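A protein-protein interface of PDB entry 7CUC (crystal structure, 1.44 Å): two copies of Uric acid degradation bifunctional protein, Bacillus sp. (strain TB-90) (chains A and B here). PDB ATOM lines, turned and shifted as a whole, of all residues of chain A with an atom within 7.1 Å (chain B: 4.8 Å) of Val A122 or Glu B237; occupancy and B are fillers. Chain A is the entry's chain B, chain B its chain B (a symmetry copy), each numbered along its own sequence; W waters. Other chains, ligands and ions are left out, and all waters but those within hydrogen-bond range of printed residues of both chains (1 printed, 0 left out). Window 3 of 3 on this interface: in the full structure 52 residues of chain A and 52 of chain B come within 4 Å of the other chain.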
ATOM      1  N   PHE A 120      10.717 -13.473  10.015  1.00  0.00           N
ATOM      2  CA  PHE A 120      10.582 -12.918  11.352  1.00  0.00           C
ATOM      3  C   PHE A 120       9.337 -12.048  11.426  1.00  0.00           C
ATOM      4  O   PHE A 120       8.863 -11.509  10.420  1.00  0.00           O
ATOM      5  CB  PHE A 120      11.845 -12.159  11.770  1.00  0.00           C
ATOM      6  CG  PHE A 120      13.100 -13.014  11.781  1.00  0.00           C
ATOM      7  CD1 PHE A 120      13.725 -13.377  10.593  1.00  0.00           C
ATOM      8  CD2 PHE A 120      13.642 -13.473  12.979  1.00  0.00           C
ATOM      9  CE1 PHE A 120      14.881 -14.162  10.596  1.00  0.00           C
ATOM     10  CE2 PHE A 120      14.799 -14.254  12.989  1.00  0.00           C
ATOM     11  CZ  PHE A 120      15.413 -14.604  11.792  1.00  0.00           C
ATOM     12  N   ALA A 121       8.804 -11.953  12.635  1.00  0.00           N
ATOM     13  CA  ALA A 121       7.552 -11.275  12.896  1.00  0.00           C
ATOM     14  C   ALA A 121       7.666 -10.649  14.267  1.00  0.00           C
ATOM     15  O   ALA A 121       8.413 -11.122  15.127  1.00  0.00           O
ATOM     16  CB  ALA A 121       6.372 -12.247  12.855  1.00  0.00           C
ATOM     17  N   VAL A 122       6.947  -9.567  14.436  1.00  0.00           N
ATOM     18  CA  VAL A 122       6.801  -8.906  15.724  1.00  0.00           C
ATOM     19  C   VAL A 122       5.526  -9.395  16.388  1.00  0.00           C
ATOM     20  O   VAL A 122       4.439  -9.315  15.802  1.00  0.00           O
ATOM     21  CB  VAL A 122       6.773  -7.383  15.544  1.00  0.00           C
ATOM     22  CG1 VAL A 122       6.518  -6.693  16.874  1.00  0.00           C
ATOM     23  CG2 VAL A 122       8.071  -6.920  14.926  1.00  0.00           C
ATOM     24  N   LYS A 123       5.642  -9.864  17.630  1.00  0.00           N
ATOM     25  CA  LYS A 123       4.471 -10.283  18.390  1.00  0.00           C
ATOM     26  C   LYS A 123       4.851 -10.345  19.862  1.00  0.00           C
ATOM     27  O   LYS A 123       5.959 -10.769  20.205  1.00  0.00           O
ATOM     28  CB  LYS A 123       3.959 -11.638  17.897  1.00  0.00           C
ATOM     29  N   ASN A 124       3.937  -9.895  20.718  1.00  0.00           N
ATOM     30  CA  ASN A 124       4.133  -9.926  22.169  1.00  0.00           C
ATOM     31  C   ASN A 124       5.376  -9.147  22.601  1.00  0.00           C
ATOM     32  O   ASN A 124       5.997  -9.453  23.628  1.00  0.00           O
ATOM     33  CB  ASN A 124       4.135 -11.361  22.706  1.00  0.00           C
ATOM     34  CG  ASN A 124       2.740 -11.977  22.723  1.00  0.00           C
ATOM     35  N   GLY A 125       5.725  -8.114  21.839  1.00  0.00           N
ATOM     36  CA  GLY A 125       6.740  -7.161  22.239  1.00  0.00           C
ATOM     37  C   GLY A 125       8.067  -7.273  21.529  1.00  0.00           C
ATOM     38  O   GLY A 125       8.884  -6.350  21.650  1.00  0.00           O
ATOM     39  N   ASN A 126       8.333  -8.353  20.800  1.00  0.00           N
ATOM     40  CA  ASN A 126       9.635  -8.432  20.165  1.00  0.00           C
ATOM     41  C   ASN A 126       9.589  -9.207  18.857  1.00  0.00           C
ATOM     42  O   ASN A 126       8.688 -10.005  18.590  1.00  0.00           O
ATOM     43  CB  ASN A 126      10.708  -8.994  21.115  1.00  0.00           C
ATOM     44  CG  ASN A 126      10.486 -10.451  21.453  1.00  0.00           C
ATOM     45  OD1 ASN A 126       9.378 -10.960  21.362  1.00  0.00           O
ATOM     46  ND2 ASN A 126      11.555 -11.128  21.860  1.00  0.00           N
ATOM     47  N   ARG A 127      10.609  -8.947  18.054  1.00  0.00           N
ATOM     48  CA  ARG A 127      10.781  -9.587  16.767  1.00  0.00           C
ATOM     49  C   ARG A 127      11.512 -10.902  16.961  1.00  0.00           C
ATOM     50  O   ARG A 127      12.571 -10.944  17.604  1.00  0.00           O
ATOM     51  CB  ARG A 127      11.610  -8.678  15.876  1.00  0.00           C
ATOM     52  CG  ARG A 127      11.582  -9.060  14.434  1.00  0.00           C
ATOM     53  CD  ARG A 127      12.219  -7.946  13.617  1.00  0.00           C
ATOM     54  NE  ARG A 127      12.151  -8.270  12.199  1.00  0.00           N
ATOM     55  CZ  ARG A 127      13.004  -9.056  11.558  1.00  0.00           C
ATOM     56  NH1 ARG A 127      14.046  -9.586  12.196  1.00  0.00           N
ATOM     57  NH2 ARG A 127      12.840  -9.269  10.264  1.00  0.00           N
ATOM     58  N   ALA A 128      10.953 -11.961  16.400  1.00  0.00           N
ATOM     59  CA  ALA A 128      11.497 -13.300  16.563  1.00  0.00           C
ATOM     60  C   ALA A 128      11.158 -14.136  15.341  1.00  0.00           C
ATOM     61  O   ALA A 128      10.271 -13.796  14.553  1.00  0.00           O
ATOM     62  CB  ALA A 128      10.927 -13.964  17.818  1.00  0.00           C
ATOM     63  N   LEU A 132       5.425 -20.043  11.636  1.00  0.00           N
ATOM     64  CA  LEU A 132       4.340 -20.218  10.673  1.00  0.00           C
ATOM     65  C   LEU A 132       4.643 -19.760   9.255  1.00  0.00           C
ATOM     66  O   LEU A 132       4.116 -20.370   8.302  1.00  0.00           O
ATOM     67  CB  LEU A 132       3.093 -19.459  11.142  1.00  0.00           C
ATOM     68  CG  LEU A 132       2.590 -19.770  12.543  1.00  0.00           C
ATOM     69  CD1 LEU A 132       1.462 -18.821  12.870  1.00  0.00           C
ATOM     70  CD2 LEU A 132       2.152 -21.219  12.589  1.00  0.00           C
ATOM     71  N   VAL A 133       5.395 -18.669   9.078  1.00  0.00           N
ATOM     72  CA  VAL A 133       5.619 -18.045   7.770  1.00  0.00           C
ATOM     73  C   VAL A 133       7.027 -18.368   7.271  1.00  0.00           C
ATOM     74  O   VAL A 133       8.015 -18.120   7.979  1.00  0.00           O
ATOM     75  CB  VAL A 133       5.370 -16.528   7.831  1.00  0.00           C
ATOM     76  CG1 VAL A 133       5.678 -15.913   6.490  1.00  0.00           C
ATOM     77  CG2 VAL A 133       3.953 -16.227   8.245  1.00  0.00           C
ATOM     78  N   PRO B  27       9.915  -1.091  13.784  1.00  0.00           N
ATOM     79  CA  PRO B  27       9.874  -2.305  14.625  1.00  0.00           C
ATOM     80  C   PRO B  27       9.958  -3.611  13.859  1.00  0.00           C
ATOM     81  O   PRO B  27      10.521  -4.587  14.368  1.00  0.00           O
ATOM     82  CB  PRO B  27       8.543  -2.180  15.375  1.00  0.00           C
ATOM     83  CG  PRO B  27       8.197  -0.741  15.331  1.00  0.00           C
ATOM     84  CD  PRO B  27       8.799  -0.173  14.071  1.00  0.00           C
ATOM     85  N   GLU B  28       9.374  -3.678  12.664  1.00  0.00           N
ATOM     86  CA  GLU B  28       9.293  -4.934  11.940  1.00  0.00           C
ATOM     87  C   GLU B  28      10.605  -5.349  11.260  1.00  0.00           C
ATOM     88  O   GLU B  28      10.687  -6.475  10.746  1.00  0.00           O
ATOM     89  CB  GLU B  28       8.212  -4.810  10.862  1.00  0.00           C
ATOM     90  CG  GLU B  28       6.794  -4.793  11.360  1.00  0.00           C
ATOM     91  CD  GLU B  28       6.296  -3.432  11.850  1.00  0.00           C
ATOM     92  OE1 GLU B  28       7.001  -2.410  11.644  1.00  0.00           O
ATOM     93  OE2 GLU B  28       5.195  -3.397  12.419  1.00  0.00           O
ATOM     94  N   SER B 233       5.917  -9.948   8.709  1.00  0.00           N
ATOM     95  CA  SER B 233       5.378  -9.786  10.056  1.00  0.00           C
ATOM     96  C   SER B 233       3.857  -9.768  10.028  1.00  0.00           C
ATOM     97  O   SER B 233       3.197 -10.505  10.783  1.00  0.00           O
ATOM     98  CB  SER B 233       5.928  -8.526  10.709  1.00  0.00           C
ATOM     99  OG  SER B 233       5.596  -8.532  12.091  1.00  0.00           O
ATOM    100  N   VAL B 234       3.267  -8.990   9.120  1.00  0.00           N
ATOM    101  CA  VAL B 234       1.806  -8.891   9.086  1.00  0.00           C
ATOM    102  C   VAL B 234       1.179 -10.240   8.733  1.00  0.00           C
ATOM    103  O   VAL B 234       0.149 -10.621   9.286  1.00  0.00           O
ATOM    104  CB  VAL B 234       1.367  -7.758   8.139  1.00  0.00           C
ATOM    105  CG1 VAL B 234      -0.147  -7.730   7.994  1.00  0.00           C
ATOM    106  CG2 VAL B 234       1.902  -6.429   8.683  1.00  0.00           C
ATOM    107  N   PHE B 235       1.775 -10.973   7.779  1.00  0.00           N
ATOM    108  CA  PHE B 235       1.263 -12.292   7.407  1.00  0.00           C
ATOM    109  C   PHE B 235       1.233 -13.217   8.630  1.00  0.00           C
ATOM    110  O   PHE B 235       0.211 -13.859   8.922  1.00  0.00           O
ATOM    111  CB  PHE B 235       2.114 -12.790   6.230  1.00  0.00           C
ATOM    112  CG  PHE B 235       1.557 -13.973   5.479  1.00  0.00           C
ATOM    113  CD1 PHE B 235       0.264 -14.450   5.686  1.00  0.00           C
ATOM    114  CD2 PHE B 235       2.317 -14.542   4.458  1.00  0.00           C
ATOM    115  CE1 PHE B 235      -0.224 -15.517   4.923  1.00  0.00           C
ATOM    116  CE2 PHE B 235       1.840 -15.598   3.689  1.00  0.00           C
ATOM    117  CZ  PHE B 235       0.569 -16.094   3.928  1.00  0.00           C
ATOM    118  N   HIS B 236       2.311 -13.210   9.423  1.00  0.00           N
ATOM    119  CA  HIS B 236       2.338 -14.008  10.645  1.00  0.00           C
ATOM    120  C   HIS B 236       1.256 -13.571  11.635  1.00  0.00           C
ATOM    121  O   HIS B 236       0.554 -14.397  12.226  1.00  0.00           O
ATOM    122  CB  HIS B 236       3.689 -13.817  11.304  1.00  0.00           C
ATOM    123  CG  HIS B 236       3.843 -14.573  12.563  1.00  0.00           C
ATOM    124  ND1 HIS B 236       3.437 -14.094  13.796  1.00  0.00           N
ATOM    125  CD2 HIS B 236       4.342 -15.809  12.786  1.00  0.00           C
ATOM    126  CE1 HIS B 236       3.685 -15.007  14.716  1.00  0.00           C
ATOM    127  NE2 HIS B 236       4.245 -16.049  14.133  1.00  0.00           N
ATOM    128  N   GLU B 237       1.125 -12.260  11.828  1.00  0.00           N
ATOM    129  CA  GLU B 237       0.255 -11.709  12.863  1.00  0.00           C
ATOM    130  C   GLU B 237      -1.231 -11.912  12.564  1.00  0.00           C
ATOM    131  O   GLU B 237      -2.052 -11.863  13.491  1.00  0.00           O
ATOM    132  CB  GLU B 237       0.484 -10.195  12.949  1.00  0.00           C
ATOM    133  CG  GLU B 237       1.875  -9.730  13.402  1.00  0.00           C
ATOM    134  CD  GLU B 237       2.065  -8.211  13.248  1.00  0.00           C
ATOM    135  OE1 GLU B 237       1.248  -7.461  13.825  1.00  0.00           O
ATOM    136  OE2 GLU B 237       3.033  -7.775  12.572  1.00  0.00           O
ATOM    137  N   THR B 238      -1.603 -12.062  11.293  1.00  0.00           N
ATOM    138  CA  THR B 238      -2.994 -11.987  10.847  1.00  0.00           C
ATOM    139  C   THR B 238      -3.585 -13.374  10.639  1.00  0.00           C
ATOM    140  O   THR B 238      -2.981 -14.220   9.966  1.00  0.00           O
ATOM    141  CB  THR B 238      -3.075 -11.247   9.496  1.00  0.00           C
ATOM    142  OG1 THR B 238      -2.446  -9.962   9.594  1.00  0.00           O
ATOM    143  CG2 THR B 238      -4.517 -11.070   9.019  1.00  0.00           C
ATOM    144  N   GLU B 239      -4.770 -13.599  11.214  1.00  0.00           N
ATOM    145  CA  GLU B 239      -5.639 -14.717  10.852  1.00  0.00           C
ATOM    146  C   GLU B 239      -6.295 -14.317   9.543  1.00  0.00           C
ATOM    147  O   GLU B 239      -7.291 -13.602   9.516  1.00  0.00           O
ATOM    148  CB  GLU B 239      -6.674 -14.995  11.939  1.00  0.00           C
ATOM    149  CG  GLU B 239      -6.074 -15.053  13.317  1.00  0.00           C
ATOM    150  CD  GLU B 239      -5.069 -16.170  13.422  1.00  0.00           C
ATOM    151  OE1 GLU B 239      -3.932 -15.895  13.856  1.00  0.00           O
ATOM    152  OE2 GLU B 239      -5.423 -17.318  13.063  1.00  0.00           O
ATOM    153  N   ARG B 253      -0.162  -1.206   7.278  1.00  0.00           N
ATOM    154  CA  ARG B 253       1.039  -1.164   8.117  1.00  0.00           C
ATOM    155  C   ARG B 253       2.175  -0.384   7.446  1.00  0.00           C
ATOM    156  O   ARG B 253       2.847   0.418   8.106  1.00  0.00           O
ATOM    157  CB  ARG B 253       1.486  -2.586   8.470  1.00  0.00           C
ATOM    158  CG  ARG B 253       2.692  -2.644   9.429  1.00  0.00           C
ATOM    159  CD  ARG B 253       2.320  -2.284  10.913  1.00  0.00           C
ATOM    160  NE  ARG B 253       1.302  -3.228  11.390  1.00  0.00           N
ATOM    161  CZ  ARG B 253       1.559  -4.444  11.880  1.00  0.00           C
ATOM    162  NH1 ARG B 253       2.805  -4.875  12.056  1.00  0.00           N
ATOM    163  NH2 ARG B 253       0.556  -5.233  12.235  1.00  0.00           N
HETATM  164  O   HOH W   1       9.957  -9.145   9.907  1.00  0.00           O
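O of Glu B28 sits at hydrogen-bond distance from NE of Arg A127.
OG of Ser B233 is in hydrogen-bond range of N of Val A122, at 2.9 Å.
OE2 of Glu B28 is in salt-bridge range of NH1 of Arg B253 (2.8 Å).
The side-chain carboxylate (OE1) of Glu B237 is in salt-bridge range of the guanidinium group (NH2) of Arg B253.
The backbone carbonyl oxygen (O) of Ala A121 is in hydrogen-bond range of the backbone NH (N) of Ala A128 (3.0 Å).
The side-chain carboxylate of Glu B237 is in hydrogen-bond range of the side-chain hydroxyl of Ser B233, at 2.7 Å.
O of Phe A120 touches N of Ser B233 (3.7 Å).
Ala A121 touches Ser B233.
Ala A121 touches His B236.
O of Pro B27 touches CG2 of Val A122 (3.4 Å).
Glu B28 touches Val A122.
Glu B237 touches Val A122.
Arg A127 touches Pro B27 (CD to O, 3.8 Å).
CG2 of Val A133 touches N of His B236 (3.6 Å).
Printed residues of chain B within 4 Å of Ala A121: Ser B233 and His B236.
Of chain B, only Pro B27, Glu B28, Ser B233 and Glu B237 come within 4 Å of Val A122.
Printed residues of chain B within 4 Å of Arg A127: Pro B27 and Glu B28.
Ala A128 touches none of the printed residues of chain B.
Printed residues of chain B within 4 Å of Val A133: His B236 (3.6 Å).
Printed residues of chain A within 4 Å of Glu B28: Val A122 (3.8 Å) and Arg A127 (2.7 Å).
Glu B237 touches one residue of chain A.
Thr B238 touches none of the printed residues of chain A.
The nearest printed residue of chain B that does not touch Val A122 is His B236 (5.3 Å).
The nearest residue of chain A that does not touch Glu B237 is Ala A121 (5.2 Å).
The nearest printed residue of chain B that does not touch Phe A120 is Glu B28 (5.4 Å).
Printed residues of chain A that touch a printed residue of chain B: Phe A120, Ala A121, Val A122, Arg A127 and Val A133.
Hydrophobic or aromatic side chains of chain A within 4 Å of the printed part of chain B: Ala A121, Val A122 and Val A133.
No position is printed for both chains.
Water W1 lies within hydrogen-bond range of O of Phe A120 (2.7 Å), O of Glu B28 (2.9 Å) and NH2 of Arg A127 (2.9 Å).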
